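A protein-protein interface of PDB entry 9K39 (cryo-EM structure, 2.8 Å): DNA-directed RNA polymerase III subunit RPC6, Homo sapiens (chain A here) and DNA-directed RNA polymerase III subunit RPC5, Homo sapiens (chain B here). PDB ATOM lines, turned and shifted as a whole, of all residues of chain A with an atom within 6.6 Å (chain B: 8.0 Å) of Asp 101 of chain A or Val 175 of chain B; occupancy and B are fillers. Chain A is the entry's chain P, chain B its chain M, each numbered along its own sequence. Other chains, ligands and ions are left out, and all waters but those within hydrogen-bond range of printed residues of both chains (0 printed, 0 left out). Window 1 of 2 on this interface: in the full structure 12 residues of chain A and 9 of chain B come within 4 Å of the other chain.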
ATOM      1  N   LEU A  63       3.453   2.077 -20.589  1.00  0.00           N
ATOM      2  CA  LEU A  63       2.759   3.001 -19.705  1.00  0.00           C
ATOM      3  C   LEU A  63       1.753   3.833 -20.485  1.00  0.00           C
ATOM      4  O   LEU A  63       1.893   4.037 -21.696  1.00  0.00           O
ATOM      5  CB  LEU A  63       3.737   3.936 -18.974  1.00  0.00           C
ATOM      6  CG  LEU A  63       4.527   3.349 -17.802  1.00  0.00           C
ATOM      7  CD1 LEU A  63       5.279   4.449 -17.072  1.00  0.00           C
ATOM      8  CD2 LEU A  63       3.608   2.604 -16.844  1.00  0.00           C
ATOM      9  N   ASP A  64       0.736   4.315 -19.772  1.00  0.00           N
ATOM     10  CA  ASP A  64      -0.292   5.183 -20.325  1.00  0.00           C
ATOM     11  C   ASP A  64      -0.455   6.399 -19.425  1.00  0.00           C
ATOM     12  O   ASP A  64      -0.297   6.314 -18.203  1.00  0.00           O
ATOM     13  CB  ASP A  64      -1.634   4.450 -20.471  1.00  0.00           C
ATOM     14  CG  ASP A  64      -1.563   3.294 -21.446  1.00  0.00           C
ATOM     15  OD1 ASP A  64      -0.798   3.390 -22.428  1.00  0.00           O
ATOM     16  OD2 ASP A  64      -2.275   2.289 -21.234  1.00  0.00           O
ATOM     17  N   LEU A  65      -0.780   7.531 -20.045  1.00  0.00           N
ATOM     18  CA  LEU A  65      -0.881   8.808 -19.354  1.00  0.00           C
ATOM     19  C   LEU A  65      -2.343   9.199 -19.178  1.00  0.00           C
ATOM     20  O   LEU A  65      -3.141   9.077 -20.114  1.00  0.00           O
ATOM     21  CB  LEU A  65      -0.135   9.900 -20.122  1.00  0.00           C
ATOM     22  CG  LEU A  65      -0.184  11.308 -19.526  1.00  0.00           C
ATOM     23  CD1 LEU A  65       0.446  11.326 -18.141  1.00  0.00           C
ATOM     24  CD2 LEU A  65       0.499  12.313 -20.444  1.00  0.00           C
ATOM     25  N   ARG A  75      -0.050   4.961 -15.620  1.00  0.00           N
ATOM     26  CA  ARG A  75      -0.634   3.665 -15.312  1.00  0.00           C
ATOM     27  C   ARG A  75      -0.012   2.586 -16.187  1.00  0.00           C
ATOM     28  O   ARG A  75       0.250   2.798 -17.374  1.00  0.00           O
ATOM     29  CB  ARG A  75      -2.155   3.679 -15.512  1.00  0.00           C
ATOM     30  CG  ARG A  75      -2.856   2.420 -15.027  1.00  0.00           C
ATOM     31  CD  ARG A  75      -4.323   2.414 -15.422  1.00  0.00           C
ATOM     32  NE  ARG A  75      -4.499   2.355 -16.869  1.00  0.00           N
ATOM     33  CZ  ARG A  75      -5.681   2.296 -17.474  1.00  0.00           C
ATOM     34  NH1 ARG A  75      -6.794   2.293 -16.754  1.00  0.00           N
ATOM     35  NH2 ARG A  75      -5.749   2.242 -18.797  1.00  0.00           N
ATOM     36  N   TYR A  96      -8.555  -5.545 -27.343  1.00  0.00           N
ATOM     37  CA  TYR A  96      -9.213  -5.163 -26.097  1.00  0.00           C
ATOM     38  C   TYR A  96      -9.163  -3.659 -25.854  1.00  0.00           C
ATOM     39  O   TYR A  96     -10.021  -3.134 -25.143  1.00  0.00           O
ATOM     40  CB  TYR A  96      -8.572  -5.911 -24.924  1.00  0.00           C
ATOM     41  CG  TYR A  96      -9.317  -5.780 -23.609  1.00  0.00           C
ATOM     42  CD1 TYR A  96      -8.970  -4.803 -22.687  1.00  0.00           C
ATOM     43  CD2 TYR A  96     -10.361  -6.641 -23.293  1.00  0.00           C
ATOM     44  CE1 TYR A  96      -9.644  -4.683 -21.484  1.00  0.00           C
ATOM     45  CE2 TYR A  96     -11.039  -6.529 -22.095  1.00  0.00           C
ATOM     46  CZ  TYR A  96     -10.678  -5.549 -21.195  1.00  0.00           C
ATOM     47  OH  TYR A  96     -11.352  -5.433 -20.002  1.00  0.00           O
ATOM     48  N   GLN A  97      -8.198  -2.958 -26.455  1.00  0.00           N
ATOM     49  CA  GLN A  97      -8.098  -1.512 -26.286  1.00  0.00           C
ATOM     50  C   GLN A  97      -9.370  -0.810 -26.750  1.00  0.00           C
ATOM     51  O   GLN A  97     -10.076  -0.187 -25.946  1.00  0.00           O
ATOM     52  CB  GLN A  97      -6.879  -1.003 -27.051  1.00  0.00           C
ATOM     53  CG  GLN A  97      -6.401   0.377 -26.663  1.00  0.00           C
ATOM     54  CD  GLN A  97      -5.052   0.699 -27.281  1.00  0.00           C
ATOM     55  OE1 GLN A  97      -4.943   0.913 -28.487  1.00  0.00           O
ATOM     56  NE2 GLN A  97      -4.015   0.725 -26.452  1.00  0.00           N
ATOM     57  N   ILE A  98      -9.699  -0.918 -28.038  1.00  0.00           N
ATOM     58  CA  ILE A  98     -10.921  -0.291 -28.527  1.00  0.00           C
ATOM     59  C   ILE A  98     -12.165  -1.052 -28.074  1.00  0.00           C
ATOM     60  O   ILE A  98     -13.242  -0.452 -27.995  1.00  0.00           O
ATOM     61  CB  ILE A  98     -10.858  -0.118 -30.056  1.00  0.00           C
ATOM     62  CG1 ILE A  98      -9.853   0.980 -30.417  1.00  0.00           C
ATOM     63  CG2 ILE A  98     -12.212   0.231 -30.657  1.00  0.00           C
ATOM     64  CD1 ILE A  98      -9.704   1.210 -31.906  1.00  0.00           C
ATOM     65  N   ILE A  99     -12.049  -2.334 -27.713  1.00  0.00           N
ATOM     66  CA  ILE A  99     -13.184  -2.993 -27.063  1.00  0.00           C
ATOM     67  C   ILE A  99     -13.597  -2.219 -25.811  1.00  0.00           C
ATOM     68  O   ILE A  99     -14.772  -1.870 -25.629  1.00  0.00           O
ATOM     69  CB  ILE A  99     -12.848  -4.459 -26.739  1.00  0.00           C
ATOM     70  CG1 ILE A  99     -12.838  -5.299 -28.017  1.00  0.00           C
ATOM     71  CG2 ILE A  99     -13.851  -5.026 -25.741  1.00  0.00           C
ATOM     72  CD1 ILE A  99     -12.664  -6.781 -27.770  1.00  0.00           C
ATOM     73  N   GLU A 100     -12.626  -1.914 -24.948  1.00  0.00           N
ATOM     74  CA  GLU A 100     -12.904  -1.135 -23.743  1.00  0.00           C
ATOM     75  C   GLU A 100     -13.293   0.300 -24.087  1.00  0.00           C
ATOM     76  O   GLU A 100     -14.166   0.882 -23.433  1.00  0.00           O
ATOM     77  CB  GLU A 100     -11.689  -1.155 -22.818  1.00  0.00           C
ATOM     78  CG  GLU A 100     -11.812  -0.246 -21.606  1.00  0.00           C
ATOM     79  CD  GLU A 100     -10.563  -0.249 -20.750  1.00  0.00           C
ATOM     80  OE1 GLU A 100      -9.603  -0.966 -21.099  1.00  0.00           O
ATOM     81  OE2 GLU A 100     -10.543   0.467 -19.725  1.00  0.00           O
ATOM     82  N   ASP A 101     -12.646   0.887 -25.098  1.00  0.00           N
ATOM     83  CA  ASP A 101     -12.985   2.248 -25.504  1.00  0.00           C
ATOM     84  C   ASP A 101     -14.455   2.363 -25.888  1.00  0.00           C
ATOM     85  O   ASP A 101     -15.122   3.344 -25.541  1.00  0.00           O
ATOM     86  CB  ASP A 101     -12.093   2.690 -26.665  1.00  0.00           C
ATOM     87  CG  ASP A 101     -10.633   2.801 -26.273  1.00  0.00           C
ATOM     88  OD1 ASP A 101     -10.353   3.102 -25.092  1.00  0.00           O
ATOM     89  OD2 ASP A 101      -9.764   2.590 -27.144  1.00  0.00           O
ATOM     90  N   ALA A 102     -14.975   1.368 -26.611  1.00  0.00           N
ATOM     91  CA  ALA A 102     -16.407   1.321 -26.884  1.00  0.00           C
ATOM     92  C   ALA A 102     -17.194   1.104 -25.599  1.00  0.00           C
ATOM     93  O   ALA A 102     -18.063   1.907 -25.245  1.00  0.00           O
ATOM     94  CB  ALA A 102     -16.712   0.224 -27.903  1.00  0.00           C
ATOM     95  N   GLY A 103     -16.890   0.024 -24.881  1.00  0.00           N
ATOM     96  CA  GLY A 103     -17.469  -0.155 -23.558  1.00  0.00           C
ATOM     97  C   GLY A 103     -18.967  -0.391 -23.604  1.00  0.00           C
ATOM     98  O   GLY A 103     -19.451  -1.363 -24.196  1.00  0.00           O
ATOM     99  N   ASN A 104     -19.714   0.510 -22.963  1.00  0.00           N
ATOM    100  CA  ASN A 104     -21.152   0.311 -22.797  1.00  0.00           C
ATOM    101  C   ASN A 104     -21.901   0.383 -24.120  1.00  0.00           C
ATOM    102  O   ASN A 104     -22.863  -0.368 -24.324  1.00  0.00           O
ATOM    103  CB  ASN A 104     -21.713   1.342 -21.816  1.00  0.00           C
ATOM    104  CG  ASN A 104     -21.519   2.770 -22.292  1.00  0.00           C
ATOM    105  OD1 ASN A 104     -20.555   3.076 -22.997  1.00  0.00           O
ATOM    106  ND2 ASN A 104     -22.434   3.652 -21.909  1.00  0.00           N
ATOM    107  N   LEU A 152     -17.439  -4.996 -22.714  1.00  0.00           N
ATOM    108  CA  LEU A 152     -16.724  -5.548 -21.574  1.00  0.00           C
ATOM    109  C   LEU A 152     -17.674  -6.363 -20.702  1.00  0.00           C
ATOM    110  O   LEU A 152     -18.834  -5.992 -20.505  1.00  0.00           O
ATOM    111  CB  LEU A 152     -16.082  -4.432 -20.752  1.00  0.00           C
ATOM    112  CG  LEU A 152     -15.014  -3.597 -21.456  1.00  0.00           C
ATOM    113  CD1 LEU A 152     -14.361  -2.632 -20.482  1.00  0.00           C
ATOM    114  CD2 LEU A 152     -13.976  -4.490 -22.108  1.00  0.00           C
ATOM    115  N   GLN B 172     -10.257  11.718 -21.083  1.00  0.00           N
ATOM    116  CA  GLN B 172     -10.623  10.327 -21.316  1.00  0.00           C
ATOM    117  C   GLN B 172      -9.512   9.627 -22.083  1.00  0.00           C
ATOM    118  O   GLN B 172      -8.820  10.239 -22.902  1.00  0.00           O
ATOM    119  CB  GLN B 172     -11.942  10.252 -22.090  1.00  0.00           C
ATOM    120  CG  GLN B 172     -12.497   8.845 -22.264  1.00  0.00           C
ATOM    121  CD  GLN B 172     -13.751   8.813 -23.115  1.00  0.00           C
ATOM    122  OE1 GLN B 172     -14.217   9.848 -23.591  1.00  0.00           O
ATOM    123  NE2 GLN B 172     -14.303   7.622 -23.313  1.00  0.00           N
ATOM    124  N   ILE B 173      -9.339   8.333 -21.820  1.00  0.00           N
ATOM    125  CA  ILE B 173      -8.178   7.632 -22.350  1.00  0.00           C
ATOM    126  C   ILE B 173      -8.407   7.379 -23.833  1.00  0.00           C
ATOM    127  O   ILE B 173      -9.041   6.391 -24.221  1.00  0.00           O
ATOM    128  CB  ILE B 173      -7.926   6.317 -21.591  1.00  0.00           C
ATOM    129  CG1 ILE B 173      -8.309   6.472 -20.120  1.00  0.00           C
ATOM    130  CG2 ILE B 173      -6.467   5.907 -21.713  1.00  0.00           C
ATOM    131  CD1 ILE B 173      -8.143   5.209 -19.309  1.00  0.00           C
ATOM    132  N   THR B 174      -7.901   8.283 -24.664  1.00  0.00           N
ATOM    133  CA  THR B 174      -8.019   8.177 -26.116  1.00  0.00           C
ATOM    134  C   THR B 174      -6.760   7.575 -26.733  1.00  0.00           C
ATOM    135  O   THR B 174      -6.185   8.111 -27.680  1.00  0.00           O
ATOM    136  CB  THR B 174      -8.320   9.546 -26.716  1.00  0.00           C
ATOM    137  OG1 THR B 174      -7.256  10.452 -26.401  1.00  0.00           O
ATOM    138  CG2 THR B 174      -9.628  10.096 -26.161  1.00  0.00           C
ATOM    139  N   VAL B 175      -6.325   6.443 -26.185  1.00  0.00           N
ATOM    140  CA  VAL B 175      -5.176   5.734 -26.736  1.00  0.00           C
ATOM    141  C   VAL B 175      -5.608   5.036 -28.018  1.00  0.00           C
ATOM    142  O   VAL B 175      -6.419   4.102 -27.994  1.00  0.00           O
ATOM    143  CB  VAL B 175      -4.604   4.742 -25.717  1.00  0.00           C
ATOM    144  CG1 VAL B 175      -3.515   5.403 -24.885  1.00  0.00           C
ATOM    145  CG2 VAL B 175      -5.711   4.218 -24.816  1.00  0.00           C
ATOM    146  N   ARG B 176      -5.073   5.492 -29.147  1.00  0.00           N
ATOM    147  CA  ARG B 176      -5.467   4.971 -30.447  1.00  0.00           C
ATOM    148  C   ARG B 176      -4.709   3.691 -30.768  1.00  0.00           C
ATOM    149  O   ARG B 176      -3.594   3.464 -30.289  1.00  0.00           O
ATOM    150  CB  ARG B 176      -5.214   6.007 -31.545  1.00  0.00           C
ATOM    151  CG  ARG B 176      -6.116   7.229 -31.476  1.00  0.00           C
ATOM    152  CD  ARG B 176      -5.879   8.140 -32.671  1.00  0.00           C
ATOM    153  NE  ARG B 176      -6.837   9.238 -32.728  1.00  0.00           N
ATOM    154  CZ  ARG B 176      -6.890  10.131 -33.711  1.00  0.00           C
ATOM    155  NH1 ARG B 176      -6.036  10.055 -34.722  1.00  0.00           N
ATOM    156  NH2 ARG B 176      -7.796  11.098 -33.683  1.00  0.00           N
ATOM    157  N   PHE B 177      -5.341   2.845 -31.577  1.00  0.00           N
ATOM    158  CA  PHE B 177      -4.693   1.631 -32.051  1.00  0.00           C
ATOM    159  C   PHE B 177      -3.462   1.973 -32.875  1.00  0.00           C
ATOM    160  O   PHE B 177      -3.522   2.796 -33.792  1.00  0.00           O
ATOM    161  CB  PHE B 177      -5.662   0.803 -32.895  1.00  0.00           C
ATOM    162  CG  PHE B 177      -6.630  -0.016 -32.093  1.00  0.00           C
ATOM    163  CD1 PHE B 177      -6.558  -0.051 -30.713  1.00  0.00           C
ATOM    164  CD2 PHE B 177      -7.605  -0.770 -32.727  1.00  0.00           C
ATOM    165  CE1 PHE B 177      -7.448  -0.807 -29.981  1.00  0.00           C
ATOM    166  CE2 PHE B 177      -8.495  -1.534 -32.002  1.00  0.00           C
ATOM    167  CZ  PHE B 177      -8.415  -1.555 -30.628  1.00  0.00           C
ATOM    168  N   SER B 178      -2.337   1.336 -32.548  1.00  0.00           N
ATOM    169  CA  SER B 178      -1.154   1.389 -33.403  1.00  0.00           C
ATOM    170  C   SER B 178      -1.417   0.457 -34.581  1.00  0.00           C
ATOM    171  O   SER B 178      -0.893  -0.658 -34.669  1.00  0.00           O
ATOM    172  CB  SER B 178       0.101   0.997 -32.630  1.00  0.00           C
ATOM    173  OG  SER B 178       0.018  -0.338 -32.163  1.00  0.00           O
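O of Arg 176 of chain B sits close to OE1 of Gln 97 of chain A (3.4 Å).
The backbone NH of Asp 64 of chain A is in hydrogen-bond range of the backbone carbonyl oxygen of Arg 75 of chain A, 2.9 Å away.
Among the printed residues, pairs that only touch across the chains: Arg 75 of chain A with Ile 173 of chain B (3.8 Å), Gln 97 of chain A with Val 175 of chain B (3.5 Å), Gln 97 of chain A with Phe 177 of chain B (2.9 Å), Ile 98 of chain A with Phe 177 of chain B (2.9 Å), Asp 101 of chain A with Ile 173 of chain B (3.6 Å) and Asp 101 of chain A with Val 175 of chain B (3.8 Å).
Printed residues of chain B within 4 Å of Asp 101 of chain A: Ile 173 and Val 175.
Of the printed residues of chain A, Arg 176 of chain B touches Gln 97 (3.4 Å).
Printed residues of chain A within 4 Å of Phe 177 of chain B: Gln 97 (2.9 Å) and Ile 98 (2.9 Å).
Of the printed residues of chain B, Gln 97 of chain A touches Val 175, Arg 176 and Phe 177.
Printed residues of chain B within 4 Å of Ile 98 of chain A: Phe 177 (2.9 Å).
The nearest residue of chain B that does not touch Asp 101 of chain A is Gln 172 of chain B (4.9 Å).
The nearest residue of chain A that does not touch Val 175 of chain B is Asp 64 of chain A (4.2 Å).
The nearest printed residue of chain A that does not touch Ile 173 of chain B is Leu 65 of chain A (4.9 Å).
Of the 14 printed residues of chain A, 4 touch a printed residue of chain B.
Hydrophobic or aromatic side chains of chain A that line the printed part of chain B: Ile 98.
Printed residues of chain B that touch a printed residue of chain A: Ile 173, Val 175, Arg 176 and Phe 177.
Hydrophobic or aromatic side chains of chain B within 4 Å of the printed part of chain A: Ile 173 and Phe 177.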
